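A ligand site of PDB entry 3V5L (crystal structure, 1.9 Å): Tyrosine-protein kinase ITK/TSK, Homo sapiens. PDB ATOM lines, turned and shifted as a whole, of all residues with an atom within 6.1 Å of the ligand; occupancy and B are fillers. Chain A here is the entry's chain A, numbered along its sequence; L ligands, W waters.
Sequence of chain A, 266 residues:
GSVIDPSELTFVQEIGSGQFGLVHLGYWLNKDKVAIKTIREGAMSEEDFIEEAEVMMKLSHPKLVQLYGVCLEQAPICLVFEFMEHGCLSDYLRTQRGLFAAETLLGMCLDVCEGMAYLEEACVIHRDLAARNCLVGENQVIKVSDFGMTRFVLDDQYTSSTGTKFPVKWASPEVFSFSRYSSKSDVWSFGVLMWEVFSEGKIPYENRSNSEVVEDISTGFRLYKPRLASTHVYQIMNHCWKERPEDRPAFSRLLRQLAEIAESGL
A nitrogen (N3) of the ligand is in hydrogen-bond range of the backbone NH (N) of Met 84 (3.0 Å). O of Met 84 is in hydrogen-bond range of N1 of the ligand, at 2.9 Å. O of Glu 85 sits at hydrogen-bond distance from O2 of the ligand. A nitrogen (N2) of the ligand sits at hydrogen-bond distance from the backbone carbonyl oxygen (O) of Glu 82, at 3.0 Å.
N of Ala 35 lies within hydrogen-bond range of O of Phe 81, at 2.9 Å. The side-chain sulfur (SG) of Cys 88 sits at hydrogen-bond distance from the side-chain carboxylate (OD1) of Asp 91 (3.5 Å). N of Ile 15 is in hydrogen-bond range of O of Val 23, 2.8 Å away. N of Val 23 sits at hydrogen-bond distance from O of Gly 16.
Ile 15 touches the ligand. CA of Gly 16 touches C5 of the ligand, 3.8 Å away. Val 23 touches the ligand (CG1 to C6, 3.6 Å). Ala 35 touches the ligand (CB to N2, 3.4 Å). Phe 81 touches the ligand. Phe 83 touches the ligand (CE1 to N1, 3.4 Å). His 86 touches the ligand (C to C15, 3.6 Å). Gly 87 touches the ligand. N of Cys 88 touches C4 of the ligand (3.6 Å). Leu 135 touches the ligand (CD2 to C4, 3.5 Å). Hydrophobic or aromatic side chains within 4 Å of the ligand: Ile 15, Val 23, Ala 35, Phe 81, Phe 83, Met 84 and Leu 135. Along chain A the residues within 4 Å of the ligand span positions 15 to 135.
Water W1 bridges the backbone NH of Cys 88 (3.0 Å) and the side-chain carboxylate of Asp 91 (3.2 Å).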
ATOM      1  N   ILE A  15     -17.179   0.275 -15.327  1.00  0.00           N
ATOM      2  CA  ILE A  15     -16.618   1.585 -15.690  1.00  0.00           C
ATOM      3  C   ILE A  15     -15.889   2.311 -14.555  1.00  0.00           C
ATOM      4  O   ILE A  15     -15.166   3.281 -14.811  1.00  0.00           O
ATOM      5  CB  ILE A  15     -17.638   2.484 -16.438  1.00  0.00           C
ATOM      6  CG1 ILE A  15     -18.970   2.613 -15.648  1.00  0.00           C
ATOM      7  CG2 ILE A  15     -17.852   1.974 -17.865  1.00  0.00           C
ATOM      8  CD1 ILE A  15     -19.929   3.739 -16.102  1.00  0.00           C
ATOM      9  N   GLY A  16     -16.069   1.838 -13.314  1.00  0.00           N
ATOM     10  CA  GLY A  16     -15.430   2.444 -12.151  1.00  0.00           C
ATOM     11  C   GLY A  16     -15.566   1.657 -10.867  1.00  0.00           C
ATOM     12  O   GLY A  16     -16.392   0.744 -10.759  1.00  0.00           O
ATOM     13  N   SER A  17     -14.727   2.018  -9.881  1.00  0.00           N
ATOM     14  CA  SER A  17     -14.697   1.427  -8.542  1.00  0.00           C
ATOM     15  C   SER A  17     -14.410   2.519  -7.509  1.00  0.00           C
ATOM     16  O   SER A  17     -13.615   3.423  -7.762  1.00  0.00           O
ATOM     17  CB  SER A  17     -13.641   0.322  -8.483  1.00  0.00           C
ATOM     18  OG  SER A  17     -13.814  -0.503  -7.345  1.00  0.00           O
ATOM     19  N   GLY A  18     -15.100   2.432  -6.367  1.00  0.00           N
ATOM     20  CA  GLY A  18     -14.978   3.386  -5.260  1.00  0.00           C
ATOM     21  C   GLY A  18     -15.163   2.729  -3.905  1.00  0.00           C
ATOM     22  O   GLY A  18     -15.958   3.188  -3.086  1.00  0.00           O
ATOM     23  N   GLY A  21     -18.155   0.836  -3.615  1.00  0.00           N
ATOM     24  CA  GLY A  21     -18.977   1.417  -4.674  1.00  0.00           C
ATOM     25  C   GLY A  21     -18.458   1.114  -6.069  1.00  0.00           C
ATOM     26  O   GLY A  21     -17.629   1.855  -6.604  1.00  0.00           O
ATOM     27  N   VAL A  23     -19.127   0.673 -10.168  1.00  0.00           N
ATOM     28  CA  VAL A  23     -19.988   1.289 -11.197  1.00  0.00           C
ATOM     29  C   VAL A  23     -19.905   0.558 -12.554  1.00  0.00           C
ATOM     30  O   VAL A  23     -18.800   0.337 -13.065  1.00  0.00           O
ATOM     31  CB  VAL A  23     -19.832   2.834 -11.333  1.00  0.00           C
ATOM     32  CG1 VAL A  23     -20.812   3.419 -12.344  1.00  0.00           C
ATOM     33  CG2 VAL A  23     -20.003   3.535  -9.979  1.00  0.00           C
ATOM     34  N   LEU A  25     -21.595   0.298 -16.685  1.00  0.00           N
ATOM     35  CA  LEU A  25     -22.340   0.869 -17.802  1.00  0.00           C
ATOM     36  C   LEU A  25     -23.365  -0.207 -18.120  1.00  0.00           C
ATOM     37  O   LEU A  25     -23.016  -1.389 -18.190  1.00  0.00           O
ATOM     38  CB  LEU A  25     -21.424   1.130 -19.019  1.00  0.00           C
ATOM     39  CG  LEU A  25     -22.088   1.288 -20.407  1.00  0.00           C
ATOM     40  CD1 LEU A  25     -22.918   2.557 -20.504  1.00  0.00           C
ATOM     41  CD2 LEU A  25     -21.049   1.260 -21.512  1.00  0.00           C
ATOM     42  N   ALA A  35     -25.891   4.198 -15.524  1.00  0.00           N
ATOM     43  CA  ALA A  35     -24.680   3.976 -14.756  1.00  0.00           C
ATOM     44  C   ALA A  35     -25.152   3.317 -13.459  1.00  0.00           C
ATOM     45  O   ALA A  35     -25.771   3.970 -12.606  1.00  0.00           O
ATOM     46  CB  ALA A  35     -23.976   5.283 -14.471  1.00  0.00           C
ATOM     47  N   LYS A  37     -24.677   1.741  -9.942  1.00  0.00           N
ATOM     48  CA  LYS A  37     -23.766   1.830  -8.811  1.00  0.00           C
ATOM     49  C   LYS A  37     -24.136   0.804  -7.726  1.00  0.00           C
ATOM     50  O   LYS A  37     -25.076   1.029  -6.969  1.00  0.00           O
ATOM     51  CB  LYS A  37     -23.725   3.267  -8.248  1.00  0.00           C
ATOM     52  CG  LYS A  37     -22.618   3.511  -7.227  1.00  0.00           C
ATOM     53  CD  LYS A  37     -22.686   4.904  -6.631  1.00  0.00           C
ATOM     54  CE  LYS A  37     -21.605   5.134  -5.606  1.00  0.00           C
ATOM     55  NZ  LYS A  37     -21.758   6.452  -4.934  1.00  0.00           N
ATOM     56  N   VAL A  65     -26.778  15.518 -10.811  1.00  0.00           N
ATOM     57  CA  VAL A  65     -27.033  14.191 -11.385  1.00  0.00           C
ATOM     58  C   VAL A  65     -28.426  13.642 -11.023  1.00  0.00           C
ATOM     59  O   VAL A  65     -28.934  13.918  -9.935  1.00  0.00           O
ATOM     60  CB  VAL A  65     -25.888  13.178 -11.112  1.00  0.00           C
ATOM     61  CG1 VAL A  65     -25.958  12.602  -9.696  1.00  0.00           C
ATOM     62  CG2 VAL A  65     -25.869  12.055 -12.148  1.00  0.00           C
ATOM     63  N   PHE A  81     -28.440   5.300 -11.914  1.00  0.00           N
ATOM     64  CA  PHE A  81     -28.202   6.685 -12.300  1.00  0.00           C
ATOM     65  C   PHE A  81     -28.271   6.863 -13.807  1.00  0.00           C
ATOM     66  O   PHE A  81     -28.074   5.900 -14.555  1.00  0.00           O
ATOM     67  CB  PHE A  81     -26.789   7.125 -11.854  1.00  0.00           C
ATOM     68  CG  PHE A  81     -26.589   7.384 -10.385  1.00  0.00           C
ATOM     69  CD1 PHE A  81     -26.092   6.388  -9.554  1.00  0.00           C
ATOM     70  CD2 PHE A  81     -26.832   8.642  -9.832  1.00  0.00           C
ATOM     71  CE1 PHE A  81     -25.877   6.630  -8.194  1.00  0.00           C
ATOM     72  CE2 PHE A  81     -26.617   8.883  -8.473  1.00  0.00           C
ATOM     73  CZ  PHE A  81     -26.145   7.867  -7.656  1.00  0.00           C
ATOM     74  N   GLU A  82     -28.467   8.117 -14.254  1.00  0.00           N
ATOM     75  CA  GLU A  82     -28.409   8.467 -15.668  1.00  0.00           C
ATOM     76  C   GLU A  82     -26.935   8.293 -16.101  1.00  0.00           C
ATOM     77  O   GLU A  82     -26.029   8.468 -15.273  1.00  0.00           O
ATOM     78  CB  GLU A  82     -28.871   9.929 -15.896  1.00  0.00           C
ATOM     79  CG  GLU A  82     -27.999  11.003 -15.243  1.00  0.00           C
ATOM     80  CD  GLU A  82     -28.302  12.437 -15.585  1.00  0.00           C
ATOM     81  OE1 GLU A  82     -28.572  12.735 -16.778  1.00  0.00           O
ATOM     82  OE2 GLU A  82     -28.205  13.294 -14.678  1.00  0.00           O
ATOM     83  N   PHE A  83     -26.702   7.920 -17.364  1.00  0.00           N
ATOM     84  CA  PHE A  83     -25.341   7.750 -17.833  1.00  0.00           C
ATOM     85  C   PHE A  83     -24.736   9.080 -18.286  1.00  0.00           C
ATOM     86  O   PHE A  83     -25.334   9.785 -19.107  1.00  0.00           O
ATOM     87  CB  PHE A  83     -25.253   6.670 -18.935  1.00  0.00           C
ATOM     88  CG  PHE A  83     -23.852   6.454 -19.462  1.00  0.00           C
ATOM     89  CD1 PHE A  83     -22.891   5.815 -18.675  1.00  0.00           C
ATOM     90  CD2 PHE A  83     -23.483   6.917 -20.716  1.00  0.00           C
ATOM     91  CE1 PHE A  83     -21.588   5.645 -19.146  1.00  0.00           C
ATOM     92  CE2 PHE A  83     -22.175   6.738 -21.184  1.00  0.00           C
ATOM     93  CZ  PHE A  83     -21.236   6.095 -20.407  1.00  0.00           C
ATOM     94  N   MET A  84     -23.563   9.420 -17.739  1.00  0.00           N
ATOM     95  CA  MET A  84     -22.843  10.637 -18.088  1.00  0.00           C
ATOM     96  C   MET A  84     -21.691  10.253 -19.008  1.00  0.00           C
ATOM     97  O   MET A  84     -20.777   9.528 -18.595  1.00  0.00           O
ATOM     98  CB  MET A  84     -22.381  11.399 -16.835  1.00  0.00           C
ATOM     99  CG  MET A  84     -23.544  11.942 -16.001  1.00  0.00           C
ATOM    100  SD  MET A  84     -24.475  13.265 -16.815  1.00  0.00           S
ATOM    101  CE  MET A  84     -23.409  14.656 -16.508  1.00  0.00           C
ATOM    102  N   GLU A  85     -21.790  10.678 -20.282  1.00  0.00           N
ATOM    103  CA  GLU A  85     -20.871  10.366 -21.390  1.00  0.00           C
ATOM    104  C   GLU A  85     -19.376  10.462 -21.122  1.00  0.00           C
ATOM    105  O   GLU A  85     -18.623   9.612 -21.621  1.00  0.00           O
ATOM    106  CB  GLU A  85     -21.234  11.182 -22.654  1.00  0.00           C
ATOM    107  CG  GLU A  85     -22.512  10.735 -23.358  1.00  0.00           C
ATOM    108  CD  GLU A  85     -22.450   9.442 -24.146  1.00  0.00           C
ATOM    109  OE1 GLU A  85     -21.570   9.311 -25.020  1.00  0.00           O
ATOM    110  OE2 GLU A  85     -23.323   8.567 -23.915  1.00  0.00           O
ATOM    111  N   HIS A  86     -18.918  11.495 -20.382  1.00  0.00           N
ATOM    112  CA  HIS A  86     -17.487  11.677 -20.145  1.00  0.00           C
ATOM    113  C   HIS A  86     -16.963  11.318 -18.735  1.00  0.00           C
ATOM    114  O   HIS A  86     -15.851  11.713 -18.377  1.00  0.00           O
ATOM    115  CB  HIS A  86     -17.007  13.055 -20.628  1.00  0.00           C
ATOM    116  CG  HIS A  86     -17.227  13.288 -22.094  1.00  0.00           C
ATOM    117  ND1 HIS A  86     -16.436  12.672 -23.039  1.00  0.00           N
ATOM    118  CD2 HIS A  86     -18.127  14.072 -22.716  1.00  0.00           C
ATOM    119  CE1 HIS A  86     -16.889  13.099 -24.206  1.00  0.00           C
ATOM    120  NE2 HIS A  86     -17.906  13.945 -24.061  1.00  0.00           N
ATOM    121  N   GLY A  87     -17.749  10.543 -17.987  1.00  0.00           N
ATOM    122  CA  GLY A  87     -17.391  10.065 -16.657  1.00  0.00           C
ATOM    123  C   GLY A  87     -17.143  11.149 -15.612  1.00  0.00           C
ATOM    124  O   GLY A  87     -17.684  12.249 -15.720  1.00  0.00           O
ATOM    125  N   CYS A  88     -16.320  10.824 -14.597  1.00  0.00           N
ATOM    126  CA  CYS A  88     -16.032  11.780 -13.529  1.00  0.00           C
ATOM    127  C   CYS A  88     -15.086  12.898 -13.966  1.00  0.00           C
ATOM    128  O   CYS A  88     -14.196  12.684 -14.780  1.00  0.00           O
ATOM    129  CB  CYS A  88     -15.602  11.102 -12.235  1.00  0.00           C
ATOM    130  SG  CYS A  88     -13.821  10.750 -12.106  1.00  0.00           S
ATOM    131  N   ASP A  91     -11.022  12.531 -13.597  1.00  0.00           N
ATOM    132  CA  ASP A  91     -10.415  11.734 -14.666  1.00  0.00           C
ATOM    133  C   ASP A  91     -10.421  12.491 -15.996  1.00  0.00           C
ATOM    134  O   ASP A  91      -9.418  12.455 -16.709  1.00  0.00           O
ATOM    135  CB  ASP A  91     -11.135  10.386 -14.831  1.00  0.00           C
ATOM    136  CG  ASP A  91     -10.967   9.407 -13.686  1.00  0.00           C
ATOM    137  OD1 ASP A  91     -11.705   8.403 -13.641  1.00  0.00           O
ATOM    138  OD2 ASP A  91     -10.059   9.629 -12.832  1.00  0.00           O
ATOM    139  N   ARG A 132     -13.733  14.461  -8.148  1.00  0.00           N
ATOM    140  CA  ARG A 132     -14.034  13.019  -8.199  1.00  0.00           C
ATOM    141  C   ARG A 132     -15.535  12.747  -7.975  1.00  0.00           C
ATOM    142  O   ARG A 132     -16.002  11.649  -8.292  1.00  0.00           O
ATOM    143  CB  ARG A 132     -13.175  12.233  -7.197  1.00  0.00           C
ATOM    144  CG  ARG A 132     -13.484  12.531  -5.732  1.00  0.00           C
ATOM    145  CD  ARG A 132     -12.679  11.687  -4.765  1.00  0.00           C
ATOM    146  NE  ARG A 132     -13.130  11.906  -3.382  1.00  0.00           N
ATOM    147  CZ  ARG A 132     -12.696  12.892  -2.595  1.00  0.00           C
ATOM    148  NH1 ARG A 132     -11.795  13.760  -3.034  1.00  0.00           N
ATOM    149  NH2 ARG A 132     -13.171  13.007  -1.358  1.00  0.00           N
ATOM    150  N   ASN A 133     -16.261  13.719  -7.390  1.00  0.00           N
ATOM    151  CA  ASN A 133     -17.703  13.626  -7.109  1.00  0.00           C
ATOM    152  C   ASN A 133     -18.541  14.495  -8.054  1.00  0.00           C
ATOM    153  O   ASN A 133     -19.677  14.860  -7.739  1.00  0.00           O
ATOM    154  CB  ASN A 133     -17.993  13.916  -5.630  1.00  0.00           C
ATOM    155  CG  ASN A 133     -17.612  12.781  -4.712  1.00  0.00           C
ATOM    156  OD1 ASN A 133     -17.693  11.601  -5.067  1.00  0.00           O
ATOM    157  ND2 ASN A 133     -17.220  13.118  -3.497  1.00  0.00           N
ATOM    158  N   CYS A 134     -17.977  14.798  -9.229  1.00  0.00           N
ATOM    159  CA  CYS A 134     -18.610  15.553 -10.299  1.00  0.00           C
ATOM    160  C   CYS A 134     -18.545  14.751 -11.580  1.00  0.00           C
ATOM    161  O   CYS A 134     -17.618  13.973 -11.760  1.00  0.00           O
ATOM    162  CB  CYS A 134     -17.982  16.930 -10.451  1.00  0.00           C
ATOM    163  SG  CYS A 134     -18.366  18.070  -9.113  1.00  0.00           S
ATOM    164  N   LEU A 135     -19.558  14.901 -12.446  1.00  0.00           N
ATOM    165  CA  LEU A 135     -19.636  14.157 -13.696  1.00  0.00           C
ATOM    166  C   LEU A 135     -19.669  15.055 -14.927  1.00  0.00           C
ATOM    167  O   LEU A 135     -20.088  16.208 -14.818  1.00  0.00           O
ATOM    168  CB  LEU A 135     -20.854  13.214 -13.683  1.00  0.00           C
ATOM    169  CG  LEU A 135     -20.839  12.117 -12.607  1.00  0.00           C
ATOM    170  CD1 LEU A 135     -22.236  11.630 -12.340  1.00  0.00           C
ATOM    171  CD2 LEU A 135     -19.944  10.958 -13.009  1.00  0.00           C
ATOM    172  N   SER A 145     -22.422  15.217  -8.358  1.00  0.00           N
ATOM    173  CA  SER A 145     -22.906  13.889  -8.008  1.00  0.00           C
ATOM    174  C   SER A 145     -22.696  13.620  -6.520  1.00  0.00           C
ATOM    175  O   SER A 145     -22.048  14.420  -5.834  1.00  0.00           O
ATOM    176  CB  SER A 145     -22.210  12.833  -8.850  1.00  0.00           C
ATOM    177  OG  SER A 145     -22.832  11.565  -8.713  1.00  0.00           O
ATOM    178  N   ASP A 146     -23.271  12.500  -6.009  1.00  0.00           N
ATOM    179  CA  ASP A 146     -23.184  12.054  -4.602  1.00  0.00           C
ATOM    180  C   ASP A 146     -23.498  13.163  -3.579  1.00  0.00           C
ATOM    181  O   ASP A 146     -22.775  13.322  -2.580  1.00  0.00           O
ATOM    182  CB  ASP A 146     -21.825  11.380  -4.333  1.00  0.00           C
ATOM    183  CG  ASP A 146     -21.499  10.160  -5.170  1.00  0.00           C
ATOM    184  OD1 ASP A 146     -22.439   9.560  -5.751  1.00  0.00           O
ATOM    185  OD2 ASP A 146     -20.312   9.778  -5.235  1.00  0.00           O
HETATM  186  C1  LIG L   1     -17.665   6.900  -8.869  1.00  0.00           C
HETATM  187  O1  LIG L   1     -16.654   6.686  -9.860  1.00  0.00           O
HETATM  188  C2  LIG L   1     -17.205   6.769 -11.103  1.00  0.00           C
HETATM  189  C3  LIG L   1     -17.387   8.014 -11.706  1.00  0.00           C
HETATM  190  C4  LIG L   1     -17.929   8.089 -12.989  1.00  0.00           C
HETATM  191  C5  LIG L   1     -17.569   5.608 -11.778  1.00  0.00           C
HETATM  192  C6  LIG L   1     -18.110   5.683 -13.061  1.00  0.00           C
HETATM  193  C7  LIG L   1     -18.324   6.925 -13.652  1.00  0.00           C
HETATM  194  C8  LIG L   1     -18.844   7.022 -14.942  1.00  0.00           C
HETATM  195  C9  LIG L   1     -18.079   6.792 -16.071  1.00  0.00           C
HETATM  196  C10 LIG L   1     -16.770   6.338 -16.277  1.00  0.00           C
HETATM  197  C11 LIG L   1     -16.283   6.184 -17.575  1.00  0.00           C
HETATM  198  C12 LIG L   1     -17.096   6.485 -18.677  1.00  0.00           C
HETATM  199  C13 LIG L   1     -16.545   6.320 -20.117  1.00  0.00           C
HETATM  200  C14 LIG L   1     -15.153   6.947 -20.220  1.00  0.00           C
HETATM  201  C15 LIG L   1     -15.189   8.459 -19.937  1.00  0.00           C
HETATM  202  C16 LIG L   1     -16.452   4.835 -20.460  1.00  0.00           C
HETATM  203  C17 LIG L   1     -17.830   4.200 -20.649  1.00  0.00           C
HETATM  204  O2  LIG L   1     -17.408   6.962 -21.071  1.00  0.00           O
HETATM  205  C18 LIG L   1     -18.392   6.961 -18.466  1.00  0.00           C
HETATM  206  C19 LIG L   1     -18.892   7.097 -17.163  1.00  0.00           C
HETATM  207  N1  LIG L   1     -20.060   7.520 -16.700  1.00  0.00           N
HETATM  208  C20 LIG L   1     -20.080   7.534 -15.365  1.00  0.00           C
HETATM  209  C21 LIG L   1     -21.226   7.894 -14.628  1.00  0.00           C
HETATM  210  C22 LIG L   1     -21.500   7.746 -13.276  1.00  0.00           C
HETATM  211  S1  LIG L   1     -20.974   7.303 -11.722  1.00  0.00           S
HETATM  212  C23 LIG L   1     -22.396   7.703 -10.909  1.00  0.00           C
HETATM  213  C24 LIG L   1     -23.244   8.182 -11.829  1.00  0.00           C
HETATM  214  C25 LIG L   1     -22.797   8.232 -13.101  1.00  0.00           C
HETATM  215  N2  LIG L   1     -23.210   8.593 -14.319  1.00  0.00           N
HETATM  216  N3  LIG L   1     -22.344   8.385 -15.178  1.00  0.00           N
HETATM  217  O   HOH W   1     -14.360   8.647 -15.370  1.00  0.00           O
